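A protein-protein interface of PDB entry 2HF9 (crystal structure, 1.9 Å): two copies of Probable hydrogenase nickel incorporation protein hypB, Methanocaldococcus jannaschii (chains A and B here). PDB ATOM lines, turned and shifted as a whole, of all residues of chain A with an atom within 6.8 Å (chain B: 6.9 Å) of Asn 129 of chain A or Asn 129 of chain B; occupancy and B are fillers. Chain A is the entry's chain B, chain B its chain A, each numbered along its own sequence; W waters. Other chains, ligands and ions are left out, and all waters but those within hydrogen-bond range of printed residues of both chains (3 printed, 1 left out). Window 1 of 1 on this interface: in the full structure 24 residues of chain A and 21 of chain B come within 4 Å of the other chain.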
ATOM      1  N   MET A  44       4.426  20.835  -1.564  1.00  0.00           N
ATOM      2  CA  MET A  44       3.793  20.722  -2.865  1.00  0.00           C
ATOM      3  C   MET A  44       2.293  20.578  -2.698  1.00  0.00           C
ATOM      4  O   MET A  44       1.795  20.321  -1.598  1.00  0.00           O
ATOM      5  CB  MET A  44       4.346  19.519  -3.620  1.00  0.00           C
ATOM      6  CG  MET A  44       5.781  19.693  -4.089  1.00  0.00           C
ATOM      7  SD  MET A  44       6.414  18.159  -4.777  1.00  0.00           S
ATOM      8  CE  MET A  44       6.653  17.222  -3.263  1.00  0.00           C
ATOM      9  N   GLY A  45       1.572  20.747  -3.798  1.00  0.00           N
ATOM     10  CA  GLY A  45       0.139  20.545  -3.785  1.00  0.00           C
ATOM     11  C   GLY A  45      -0.471  20.851  -5.127  1.00  0.00           C
ATOM     12  O   GLY A  45       0.238  21.208  -6.072  1.00  0.00           O
ATOM     13  N   ALA A  46      -1.791  20.696  -5.204  1.00  0.00           N
ATOM     14  CA  ALA A  46      -2.560  21.153  -6.349  1.00  0.00           C
ATOM     15  C   ALA A  46      -2.693  22.671  -6.250  1.00  0.00           C
ATOM     16  O   ALA A  46      -1.974  23.310  -5.491  1.00  0.00           O
ATOM     17  CB  ALA A  46      -3.934  20.484  -6.371  1.00  0.00           C
ATOM     18  N   ILE A  47      -3.617  23.247  -7.006  1.00  0.00           N
ATOM     19  CA  ILE A  47      -3.850  24.681  -6.959  1.00  0.00           C
ATOM     20  C   ILE A  47      -4.880  24.955  -5.864  1.00  0.00           C
ATOM     21  O   ILE A  47      -5.989  24.423  -5.907  1.00  0.00           O
ATOM     22  CB  ILE A  47      -4.356  25.214  -8.328  1.00  0.00           C
ATOM     23  CG1 ILE A  47      -3.362  24.887  -9.456  1.00  0.00           C
ATOM     24  CG2 ILE A  47      -4.641  26.703  -8.253  1.00  0.00           C
ATOM     25  CD1 ILE A  47      -3.479  23.433 -10.027  1.00  0.00           C
ATOM     26  N   LYS A  51      -1.473  25.123   0.852  1.00  0.00           N
ATOM     27  CA  LYS A  51      -0.042  25.189   1.195  1.00  0.00           C
ATOM     28  C   LYS A  51       0.301  26.418   2.038  1.00  0.00           C
ATOM     29  O   LYS A  51       0.948  26.303   3.081  1.00  0.00           O
ATOM     30  CB  LYS A  51       0.832  25.184  -0.068  1.00  0.00           C
ATOM     31  CG  LYS A  51       0.640  23.989  -0.987  1.00  0.00           C
ATOM     32  CD  LYS A  51       1.640  23.997  -2.139  1.00  0.00           C
ATOM     33  CE  LYS A  51       1.354  25.097  -3.152  1.00  0.00           C
ATOM     34  NZ  LYS A  51       0.071  24.853  -3.865  1.00  0.00           N
ATOM     35  N   GLU A  99       7.083  28.171 -15.451  1.00  0.00           N
ATOM     36  CA  GLU A  99       7.621  26.906 -14.977  1.00  0.00           C
ATOM     37  C   GLU A  99       6.640  26.180 -14.069  1.00  0.00           C
ATOM     38  O   GLU A  99       5.969  26.776 -13.223  1.00  0.00           O
ATOM     39  CB  GLU A  99       9.001  27.057 -14.328  1.00  0.00           C
ATOM     40  CG  GLU A  99       9.824  25.761 -14.307  1.00  0.00           C
ATOM     41  CD  GLU A  99       9.799  24.996 -15.631  1.00  0.00           C
ATOM     42  OE1 GLU A  99       8.856  24.194 -15.857  1.00  0.00           O
ATOM     43  OE2 GLU A  99      10.736  25.184 -16.438  1.00  0.00           O
ATOM     44  N   CYS A 100       6.580  24.872 -14.275  1.00  0.00           N
ATOM     45  CA  CYS A 100       5.590  24.010 -13.675  1.00  0.00           C
ATOM     46  C   CYS A 100       5.926  23.722 -12.208  1.00  0.00           C
ATOM     47  O   CYS A 100       5.050  23.400 -11.403  1.00  0.00           O
ATOM     48  CB  CYS A 100       5.547  22.722 -14.500  1.00  0.00           C
ATOM     49  SG  CYS A 100       4.096  21.741 -14.291  1.00  0.00           S
ATOM     50  N   HIS A 101       7.202  23.877 -11.871  1.00  0.00           N
ATOM     51  CA  HIS A 101       7.759  23.428 -10.607  1.00  0.00           C
ATOM     52  C   HIS A 101       8.920  24.343 -10.240  1.00  0.00           C
ATOM     53  O   HIS A 101       9.513  24.971 -11.116  1.00  0.00           O
ATOM     54  CB  HIS A 101       8.313  22.018 -10.800  1.00  0.00           C
ATOM     55  CG  HIS A 101       9.355  21.936 -11.874  1.00  0.00           C
ATOM     56  ND1 HIS A 101       9.039  21.818 -13.211  1.00  0.00           N
ATOM     57  CD2 HIS A 101      10.706  21.999 -11.813  1.00  0.00           C
ATOM     58  CE1 HIS A 101      10.150  21.798 -13.925  1.00  0.00           C
ATOM     59  NE2 HIS A 101      11.176  21.910 -13.101  1.00  0.00           N
ATOM     60  N   ASN A 126       6.246  25.225  -3.076  1.00  0.00           N
ATOM     61  CA  ASN A 126       6.420  24.920  -4.486  1.00  0.00           C
ATOM     62  C   ASN A 126       5.256  25.458  -5.301  1.00  0.00           C
ATOM     63  O   ASN A 126       4.227  25.843  -4.739  1.00  0.00           O
ATOM     64  CB  ASN A 126       6.520  23.404  -4.672  1.00  0.00           C
ATOM     65  CG  ASN A 126       7.518  23.009  -5.737  1.00  0.00           C
ATOM     66  OD1 ASN A 126       7.501  23.527  -6.856  1.00  0.00           O
ATOM     67  ND2 ASN A 126       8.387  22.063  -5.398  1.00  0.00           N
ATOM     68  N   VAL A 127       5.418  25.485  -6.621  1.00  0.00           N
ATOM     69  CA  VAL A 127       4.338  25.884  -7.522  1.00  0.00           C
ATOM     70  C   VAL A 127       3.195  24.869  -7.405  1.00  0.00           C
ATOM     71  O   VAL A 127       3.436  23.659  -7.395  1.00  0.00           O
ATOM     72  CB  VAL A 127       4.819  25.970  -8.991  1.00  0.00           C
ATOM     73  CG1 VAL A 127       3.781  26.672  -9.870  1.00  0.00           C
ATOM     74  CG2 VAL A 127       6.153  26.700  -9.081  1.00  0.00           C
ATOM     75  N   GLY A 128       1.966  25.371  -7.296  1.00  0.00           N
ATOM     76  CA  GLY A 128       0.775  24.517  -7.254  1.00  0.00           C
ATOM     77  C   GLY A 128       0.625  23.731  -8.543  1.00  0.00           C
ATOM     78  O   GLY A 128       0.379  24.314  -9.598  1.00  0.00           O
ATOM     79  N   ASN A 129       0.780  22.409  -8.441  1.00  0.00           N
ATOM     80  CA  ASN A 129       0.791  21.478  -9.581  1.00  0.00           C
ATOM     81  C   ASN A 129       1.087  20.055  -9.105  1.00  0.00           C
ATOM     82  O   ASN A 129       1.969  19.853  -8.264  1.00  0.00           O
ATOM     83  CB  ASN A 129       1.846  21.883 -10.621  1.00  0.00           C
ATOM     84  CG  ASN A 129       1.301  22.834 -11.680  1.00  0.00           C
ATOM     85  OD1 ASN A 129       0.122  22.781 -12.037  1.00  0.00           O
ATOM     86  ND2 ASN A 129       2.166  23.707 -12.189  1.00  0.00           N
ATOM     87  N   LEU A 130       0.369  19.073  -9.649  1.00  0.00           N
ATOM     88  CA  LEU A 130       0.540  17.676  -9.225  1.00  0.00           C
ATOM     89  C   LEU A 130       1.310  16.755 -10.182  1.00  0.00           C
ATOM     90  O   LEU A 130       1.398  15.554  -9.941  1.00  0.00           O
ATOM     91  CB  LEU A 130      -0.812  17.038  -8.869  1.00  0.00           C
ATOM     92  CG  LEU A 130      -1.529  17.475  -7.586  1.00  0.00           C
ATOM     93  CD1 LEU A 130      -2.790  16.654  -7.407  1.00  0.00           C
ATOM     94  CD2 LEU A 130      -0.645  17.358  -6.346  1.00  0.00           C
ATOM     95  N   ILE A 131       1.873  17.296 -11.254  1.00  0.00           N
ATOM     96  CA  ILE A 131       2.667  16.460 -12.161  1.00  0.00           C
ATOM     97  C   ILE A 131       4.168  16.708 -12.003  1.00  0.00           C
ATOM     98  O   ILE A 131       4.919  15.840 -11.563  1.00  0.00           O
ATOM     99  CB  ILE A 131       2.276  16.659 -13.662  1.00  0.00           C
ATOM    100  CG1 ILE A 131       0.759  16.860 -13.849  1.00  0.00           C
ATOM    101  CG2 ILE A 131       2.850  15.519 -14.524  1.00  0.00           C
ATOM    102  CD1 ILE A 131      -0.127  15.687 -13.423  1.00  0.00           C
ATOM    103  N   CYS A 132       4.571  17.924 -12.350  1.00  0.00           N
ATOM    104  CA  CYS A 132       5.965  18.311 -12.566  1.00  0.00           C
ATOM    105  C   CYS A 132       6.922  18.320 -11.366  1.00  0.00           C
ATOM    106  O   CYS A 132       8.091  17.948 -11.528  1.00  0.00           O
ATOM    107  CB  CYS A 132       5.968  19.681 -13.215  1.00  0.00           C
ATOM    108  SG  CYS A 132       4.562  20.647 -12.653  1.00  0.00           S
ATOM    109  N   PRO A 133       6.456  18.765 -10.171  1.00  0.00           N
ATOM    110  CA  PRO A 133       7.388  18.798  -9.037  1.00  0.00           C
ATOM    111  C   PRO A 133       7.844  17.404  -8.583  1.00  0.00           C
ATOM    112  O   PRO A 133       8.836  17.286  -7.859  1.00  0.00           O
ATOM    113  CB  PRO A 133       6.579  19.500  -7.937  1.00  0.00           C
ATOM    114  CG  PRO A 133       5.453  20.190  -8.660  1.00  0.00           C
ATOM    115  CD  PRO A 133       5.128  19.262  -9.772  1.00  0.00           C
ATOM    116  N   ALA A 134       7.123  16.367  -9.001  1.00  0.00           N
ATOM    117  CA  ALA A 134       7.631  15.008  -8.899  1.00  0.00           C
ATOM    118  C   ALA A 134       8.724  14.858  -9.949  1.00  0.00           C
ATOM    119  O   ALA A 134       8.465  15.024 -11.147  1.00  0.00           O
ATOM    120  CB  ALA A 134       6.530  14.003  -9.134  1.00  0.00           C
ATOM    121  N   ILE A 162       3.795  11.782  -7.998  1.00  0.00           N
ATOM    122  CA  ILE A 162       4.081  12.789  -6.976  1.00  0.00           C
ATOM    123  C   ILE A 162       3.825  12.274  -5.553  1.00  0.00           C
ATOM    124  O   ILE A 162       4.594  12.571  -4.640  1.00  0.00           O
ATOM    125  CB  ILE A 162       3.336  14.139  -7.245  1.00  0.00           C
ATOM    126  CG1 ILE A 162       3.994  15.284  -6.458  1.00  0.00           C
ATOM    127  CG2 ILE A 162       1.831  14.016  -6.963  1.00  0.00           C
ATOM    128  CD1 ILE A 162       3.539  16.685  -6.859  1.00  0.00           C
ATOM    129  N   MET B  44      -9.952  23.477 -20.012  1.00  0.00           N
ATOM    130  CA  MET B  44      -8.785  23.594 -19.147  1.00  0.00           C
ATOM    131  C   MET B  44      -9.226  23.949 -17.732  1.00  0.00           C
ATOM    132  O   MET B  44     -10.360  24.372 -17.519  1.00  0.00           O
ATOM    133  CB  MET B  44      -7.843  24.693 -19.664  1.00  0.00           C
ATOM    134  CG  MET B  44      -7.149  24.382 -20.988  1.00  0.00           C
ATOM    135  SD  MET B  44      -6.293  25.831 -21.647  1.00  0.00           S
ATOM    136  CE  MET B  44      -7.682  26.778 -22.274  1.00  0.00           C
ATOM    137  N   GLY B  45      -8.326  23.778 -16.768  1.00  0.00           N
ATOM    138  CA  GLY B  45      -8.584  24.203 -15.401  1.00  0.00           C
ATOM    139  C   GLY B  45      -7.581  23.687 -14.392  1.00  0.00           C
ATOM    140  O   GLY B  45      -6.627  22.982 -14.745  1.00  0.00           O
ATOM    141  N   ALA B  46      -7.801  24.041 -13.131  1.00  0.00           N
ATOM    142  CA  ALA B  46      -6.972  23.556 -12.034  1.00  0.00           C
ATOM    143  C   ALA B  46      -7.353  22.107 -11.710  1.00  0.00           C
ATOM    144  O   ALA B  46      -8.259  21.542 -12.331  1.00  0.00           O
ATOM    145  CB  ALA B  46      -7.139  24.447 -10.819  1.00  0.00           C
ATOM    146  N   ILE B  47      -6.669  21.498 -10.750  1.00  0.00           N
ATOM    147  CA  ILE B  47      -7.006  20.129 -10.354  1.00  0.00           C
ATOM    148  C   ILE B  47      -8.358  20.119  -9.639  1.00  0.00           C
ATOM    149  O   ILE B  47      -8.552  20.830  -8.650  1.00  0.00           O
ATOM    150  CB  ILE B  47      -5.933  19.498  -9.431  1.00  0.00           C
ATOM    151  CG1 ILE B  47      -4.562  19.434 -10.124  1.00  0.00           C
ATOM    152  CG2 ILE B  47      -6.381  18.112  -8.949  1.00  0.00           C
ATOM    153  CD1 ILE B  47      -4.376  18.266 -11.093  1.00  0.00           C
ATOM    154  N   LYS B  51     -14.168  20.094 -14.428  1.00  0.00           N
ATOM    155  CA  LYS B  51     -14.182  19.907 -15.889  1.00  0.00           C
ATOM    156  C   LYS B  51     -15.035  18.712 -16.309  1.00  0.00           C
ATOM    157  O   LYS B  51     -15.877  18.820 -17.201  1.00  0.00           O
ATOM    158  CB  LYS B  51     -12.757  19.731 -16.442  1.00  0.00           C
ATOM    159  CG  LYS B  51     -11.795  20.888 -16.175  1.00  0.00           C
ATOM    160  CD  LYS B  51     -10.424  20.671 -16.853  1.00  0.00           C
ATOM    161  CE  LYS B  51      -9.577  19.589 -16.167  1.00  0.00           C
ATOM    162  NZ  LYS B  51      -9.384  19.850 -14.714  1.00  0.00           N
ATOM    163  N   GLU B  99       3.555  14.828 -19.138  1.00  0.00           N
ATOM    164  CA  GLU B  99       3.226  16.068 -19.838  1.00  0.00           C
ATOM    165  C   GLU B  99       2.156  16.868 -19.084  1.00  0.00           C
ATOM    166  O   GLU B  99       1.136  16.321 -18.657  1.00  0.00           O
ATOM    167  CB  GLU B  99       2.776  15.766 -21.272  1.00  0.00           C
ATOM    168  CG  GLU B  99       3.243  16.786 -22.309  1.00  0.00           C
ATOM    169  CD  GLU B  99       4.758  16.922 -22.369  1.00  0.00           C
ATOM    170  OE1 GLU B  99       5.457  15.892 -22.510  1.00  0.00           O
ATOM    171  OE2 GLU B  99       5.253  18.064 -22.275  1.00  0.00           O
ATOM    172  N   CYS B 100       2.404  18.163 -18.920  1.00  0.00           N
ATOM    173  CA  CYS B 100       1.510  19.040 -18.164  1.00  0.00           C
ATOM    174  C   CYS B 100       0.484  19.746 -19.053  1.00  0.00           C
ATOM    175  O   CYS B 100      -0.106  20.756 -18.659  1.00  0.00           O
ATOM    176  CB  CYS B 100       2.323  20.061 -17.361  1.00  0.00           C
ATOM    177  SG  CYS B 100       3.473  21.032 -18.343  1.00  0.00           S
ATOM    178  N   HIS B 101       0.274  19.198 -20.249  1.00  0.00           N
ATOM    179  CA  HIS B 101      -0.665  19.740 -21.231  1.00  0.00           C
ATOM    180  C   HIS B 101      -0.886  18.720 -22.346  1.00  0.00           C
ATOM    181  O   HIS B 101      -0.021  17.884 -22.608  1.00  0.00           O
ATOM    182  CB  HIS B 101      -0.118  21.038 -21.836  1.00  0.00           C
ATOM    183  CG  HIS B 101       1.137  20.851 -22.634  1.00  0.00           C
ATOM    184  ND1 HIS B 101       2.395  20.938 -22.078  1.00  0.00           N
ATOM    185  CD2 HIS B 101       1.325  20.570 -23.946  1.00  0.00           C
ATOM    186  CE1 HIS B 101       3.304  20.726 -23.013  1.00  0.00           C
ATOM    187  NE2 HIS B 101       2.681  20.498 -24.156  1.00  0.00           N
ATOM    188  N   ASN B 126      -8.579  18.782 -21.103  1.00  0.00           N
ATOM    189  CA  ASN B 126      -7.143  18.944 -20.996  1.00  0.00           C
ATOM    190  C   ASN B 126      -6.663  18.466 -19.629  1.00  0.00           C
ATOM    191  O   ASN B 126      -7.474  18.182 -18.742  1.00  0.00           O
ATOM    192  CB  ASN B 126      -6.787  20.420 -21.191  1.00  0.00           C
ATOM    193  CG  ASN B 126      -5.484  20.618 -21.932  1.00  0.00           C
ATOM    194  OD1 ASN B 126      -4.483  19.947 -21.662  1.00  0.00           O
ATOM    195  ND2 ASN B 126      -5.484  21.559 -22.863  1.00  0.00           N
ATOM    196  N   VAL B 127      -5.351  18.378 -19.446  1.00  0.00           N
ATOM    197  CA  VAL B 127      -4.818  17.998 -18.138  1.00  0.00           C
ATOM    198  C   VAL B 127      -5.036  19.154 -17.147  1.00  0.00           C
ATOM    199  O   VAL B 127      -5.043  20.322 -17.544  1.00  0.00           O
ATOM    200  CB  VAL B 127      -3.329  17.567 -18.203  1.00  0.00           C
ATOM    201  CG1 VAL B 127      -3.047  16.720 -19.449  1.00  0.00           C
ATOM    202  CG2 VAL B 127      -2.429  18.764 -18.176  1.00  0.00           C
ATOM    203  N   GLY B 128      -5.249  18.822 -15.873  1.00  0.00           N
ATOM    204  CA  GLY B 128      -5.478  19.831 -14.832  1.00  0.00           C
ATOM    205  C   GLY B 128      -4.209  20.573 -14.458  1.00  0.00           C
ATOM    206  O   GLY B 128      -3.361  20.042 -13.743  1.00  0.00           O
ATOM    207  N   ASN B 129      -4.093  21.808 -14.948  1.00  0.00           N
ATOM    208  CA  ASN B 129      -2.886  22.623 -14.831  1.00  0.00           C
ATOM    209  C   ASN B 129      -3.224  24.010 -15.360  1.00  0.00           C
ATOM    210  O   ASN B 129      -3.799  24.132 -16.446  1.00  0.00           O
ATOM    211  CB  ASN B 129      -1.743  22.013 -15.664  1.00  0.00           C
ATOM    212  CG  ASN B 129      -0.363  22.571 -15.301  1.00  0.00           C
ATOM    213  OD1 ASN B 129      -0.107  23.772 -15.403  1.00  0.00           O
ATOM    214  ND2 ASN B 129       0.539  21.683 -14.901  1.00  0.00           N
ATOM    215  N   LEU B 130      -2.872  25.046 -14.601  1.00  0.00           N
ATOM    216  CA  LEU B 130      -3.145  26.426 -15.011  1.00  0.00           C
ATOM    217  C   LEU B 130      -1.954  27.134 -15.664  1.00  0.00           C
ATOM    218  O   LEU B 130      -2.024  28.332 -15.949  1.00  0.00           O
ATOM    219  CB  LEU B 130      -3.663  27.255 -13.825  1.00  0.00           C
ATOM    220  CG  LEU B 130      -5.096  27.042 -13.328  1.00  0.00           C
ATOM    221  CD1 LEU B 130      -5.362  27.942 -12.129  1.00  0.00           C
ATOM    222  CD2 LEU B 130      -6.133  27.296 -14.429  1.00  0.00           C
ATOM    223  N   ILE B 131      -0.872  26.398 -15.904  1.00  0.00           N
ATOM    224  CA  ILE B 131       0.346  26.974 -16.480  1.00  0.00           C
ATOM    225  C   ILE B 131       0.581  26.546 -17.936  1.00  0.00           C
ATOM    226  O   ILE B 131       0.425  27.364 -18.848  1.00  0.00           O
ATOM    227  CB  ILE B 131       1.599  26.694 -15.590  1.00  0.00           C
ATOM    228  CG1 ILE B 131       1.562  27.534 -14.311  1.00  0.00           C
ATOM    229  CG2 ILE B 131       2.888  27.013 -16.330  1.00  0.00           C
ATOM    230  CD1 ILE B 131       0.912  26.855 -13.140  1.00  0.00           C
ATOM    231  N   CYS B 132       0.926  25.272 -18.145  1.00  0.00           N
ATOM    232  CA  CYS B 132       1.371  24.767 -19.458  1.00  0.00           C
ATOM    233  C   CYS B 132       0.360  24.845 -20.607  1.00  0.00           C
ATOM    234  O   CYS B 132       0.743  25.212 -21.724  1.00  0.00           O
ATOM    235  CB  CYS B 132       1.864  23.324 -19.350  1.00  0.00           C
ATOM    236  SG  CYS B 132       2.947  22.959 -17.971  1.00  0.00           S
ATOM    237  N   PRO B 133      -0.917  24.468 -20.360  1.00  0.00           N
ATOM    238  CA  PRO B 133      -1.885  24.468 -21.463  1.00  0.00           C
ATOM    239  C   PRO B 133      -2.116  25.832 -22.123  1.00  0.00           C
ATOM    240  O   PRO B 133      -2.637  25.889 -23.237  1.00  0.00           O
ATOM    241  CB  PRO B 133      -3.177  23.974 -20.793  1.00  0.00           C
ATOM    242  CG  PRO B 133      -2.723  23.224 -19.590  1.00  0.00           C
ATOM    243  CD  PRO B 133      -1.537  23.999 -19.106  1.00  0.00           C
ATOM    244  N   ALA B 134      -1.724  26.912 -21.448  1.00  0.00           N
ATOM    245  CA  ALA B 134      -1.906  28.265 -21.974  1.00  0.00           C
ATOM    246  C   ALA B 134      -1.266  28.453 -23.350  1.00  0.00           C
ATOM    247  O   ALA B 134      -1.859  29.077 -24.234  1.00  0.00           O
ATOM    248  CB  ALA B 134      -1.364  29.294 -20.992  1.00  0.00           C
ATOM    249  N   ILE B 162      -3.001  32.088 -18.541  1.00  0.00           N
ATOM    250  CA  ILE B 162      -4.001  31.152 -19.070  1.00  0.00           C
ATOM    251  C   ILE B 162      -5.374  31.813 -19.224  1.00  0.00           C
ATOM    252  O   ILE B 162      -6.106  31.511 -20.170  1.00  0.00           O
ATOM    253  CB  ILE B 162      -4.097  29.830 -18.241  1.00  0.00           C
ATOM    254  CG1 ILE B 162      -4.814  28.733 -19.050  1.00  0.00           C
ATOM    255  CG2 ILE B 162      -4.756  30.070 -16.877  1.00  0.00           C
ATOM    256  CD1 ILE B 162      -4.743  27.339 -18.434  1.00  0.00           C
HETATM  257  O   HOH W   1      -6.488  22.541  -7.898  1.00  0.00           O
HETATM  258  O   HOH W   2      -1.334  24.850 -12.272  1.00  0.00           O
HETATM  259  O   HOH W   3      -1.123  19.039 -12.002  1.00  0.00           O
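ND2 of Asn 129 of chain B sits at hydrogen-bond distance from SG of Cys 100 of chain A, at 3.6 Å.
The side-chain amide oxygen of Asn 129 of chain A is in hydrogen-bond range of the side-chain amide nitrogen of Asn 129 of chain B (3.1 Å).
The backbone NH (N) of Asn 129 of chain B lies within hydrogen-bond range of the backbone carbonyl oxygen (O) of Gly 45 of chain B.
The backbone carbonyl oxygen (O) of Ala 46 of chain B lies within hydrogen-bond range of the side-chain amino group (NZ) of Lys 51 of chain B (3.1 Å).
The side-chain sulfur (SG) of Cys 100 of chain B is disulfide-bonded to the side-chain sulfur (SG) of Cys 132 of chain B, 2.0 Å away.
The backbone NH (N) of Ile 131 of chain B lies within hydrogen-bond range of the side-chain amide oxygen (OD1) of Asn 129 of chain B (2.8 Å).
The backbone NH (N) of Cys 132 of chain B sits at hydrogen-bond distance from the side-chain amide oxygen (OD1) of Asn 129 of chain B (3.3 Å).
The side-chain amino group of Lys 51 of chain A lies within hydrogen-bond range of the backbone carbonyl oxygen of Ala 46 of chain A (3.0 Å).
Ala 46 of chain A touches Ile 47 of chain B.
CB of Ile 47 of chain A touches CB of Ala 46 of chain B (3.8 Å).
Ile 47 of chain A touches Ile 47 of chain B.
CB of Cys 100 of chain B touches SG of Cys 100 of chain A, 3.9 Å away.
ND2 of Asn 129 of chain A touches CD1 of Ile 131 of chain B, 3.5 Å away.
Of the printed residues of chain B, Ile 47 of chain A touches Ala 46 and Ile 47.
Of the printed residues of chain B, Cys 100 of chain A touches Cys 100 and Asn 129.
Asn 129 of chain A touches just these residues of chain B: Asn 129 (3.1 Å) and Ile 131 (3.5 Å).
Of the printed residues of chain A, Ile 47 of chain B touches Ala 46 (3.8 Å) and Ile 47 (3.8 Å).
Printed residues of chain A within 4 Å of Asn 129 of chain B: Cys 100 (3.6 Å) and Asn 129 (3.1 Å).
Printed residues of chain A within 4 Å of Ile 131 of chain B: Asn 129.
The nearest residue of chain A that does not touch Asn 129 of chain B is Cys 132 of chain A (4.7 Å).
The nearest printed residue of chain B that does not touch Cys 100 of chain A is Cys 132 of chain B (4.04 Å).
Hydrophobic or aromatic side chains of chain B that line the printed part of chain A: Ala 46, Ile 47 and Ile 131.
Of the 18 printed residues of chain A, 4 touch a printed residue of chain B.
Along chain A the printed residues that touch a printed residue of chain B span positions 46 to 129.
Among the printed residues, 7 pairs touch across the chains.
Among the printed residues, no Asp or Glu carboxylate lies within 4 Å of a Lys or Arg side-chain nitrogen of the other chain.
Ala 46 of chain A touches Ile 47 of chain B, and with the chains exchanged Ile 47 of chain A touches Ala 46 of chain B.
Cys 100 of chain A touches its own counterpart, Cys 100 of chain B.
Cys 100 of chain A touches Asn 129 of chain B, but with the chains exchanged Asn 129 of chain A does not touch Cys 100 of chain B (6.3 Å).
Asn 129 of chain A touches its own counterpart, Asn 129 of chain B.
Positions printed for both chains: 44, 45, 46, 47, 51, 99, 100, 101, 126, 127, 128, 129, 130, 131, 132, 133, 134 and 162.
Of the 7 pairs that touch across the chains among the printed residues, 5 have their exchanged pair printed and touching as well.
Water W2 lies within hydrogen-bond range of the side-chain amide oxygen of Asn 129 of chain A (2.5 Å), the backbone NH of Leu 130 of chain B (2.8 Å) and the backbone carbonyl oxygen of Gly 128 of chain A (3.2 Å).
Water W1 lies within hydrogen-bond range of O of Ile 47 of chain A and O of Ile 47 of chain B.
Water W3 lies within hydrogen-bond range of N of Leu 130 of chain A (2.8 Å) and O of Gly 128 of chain B (3.0 Å).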
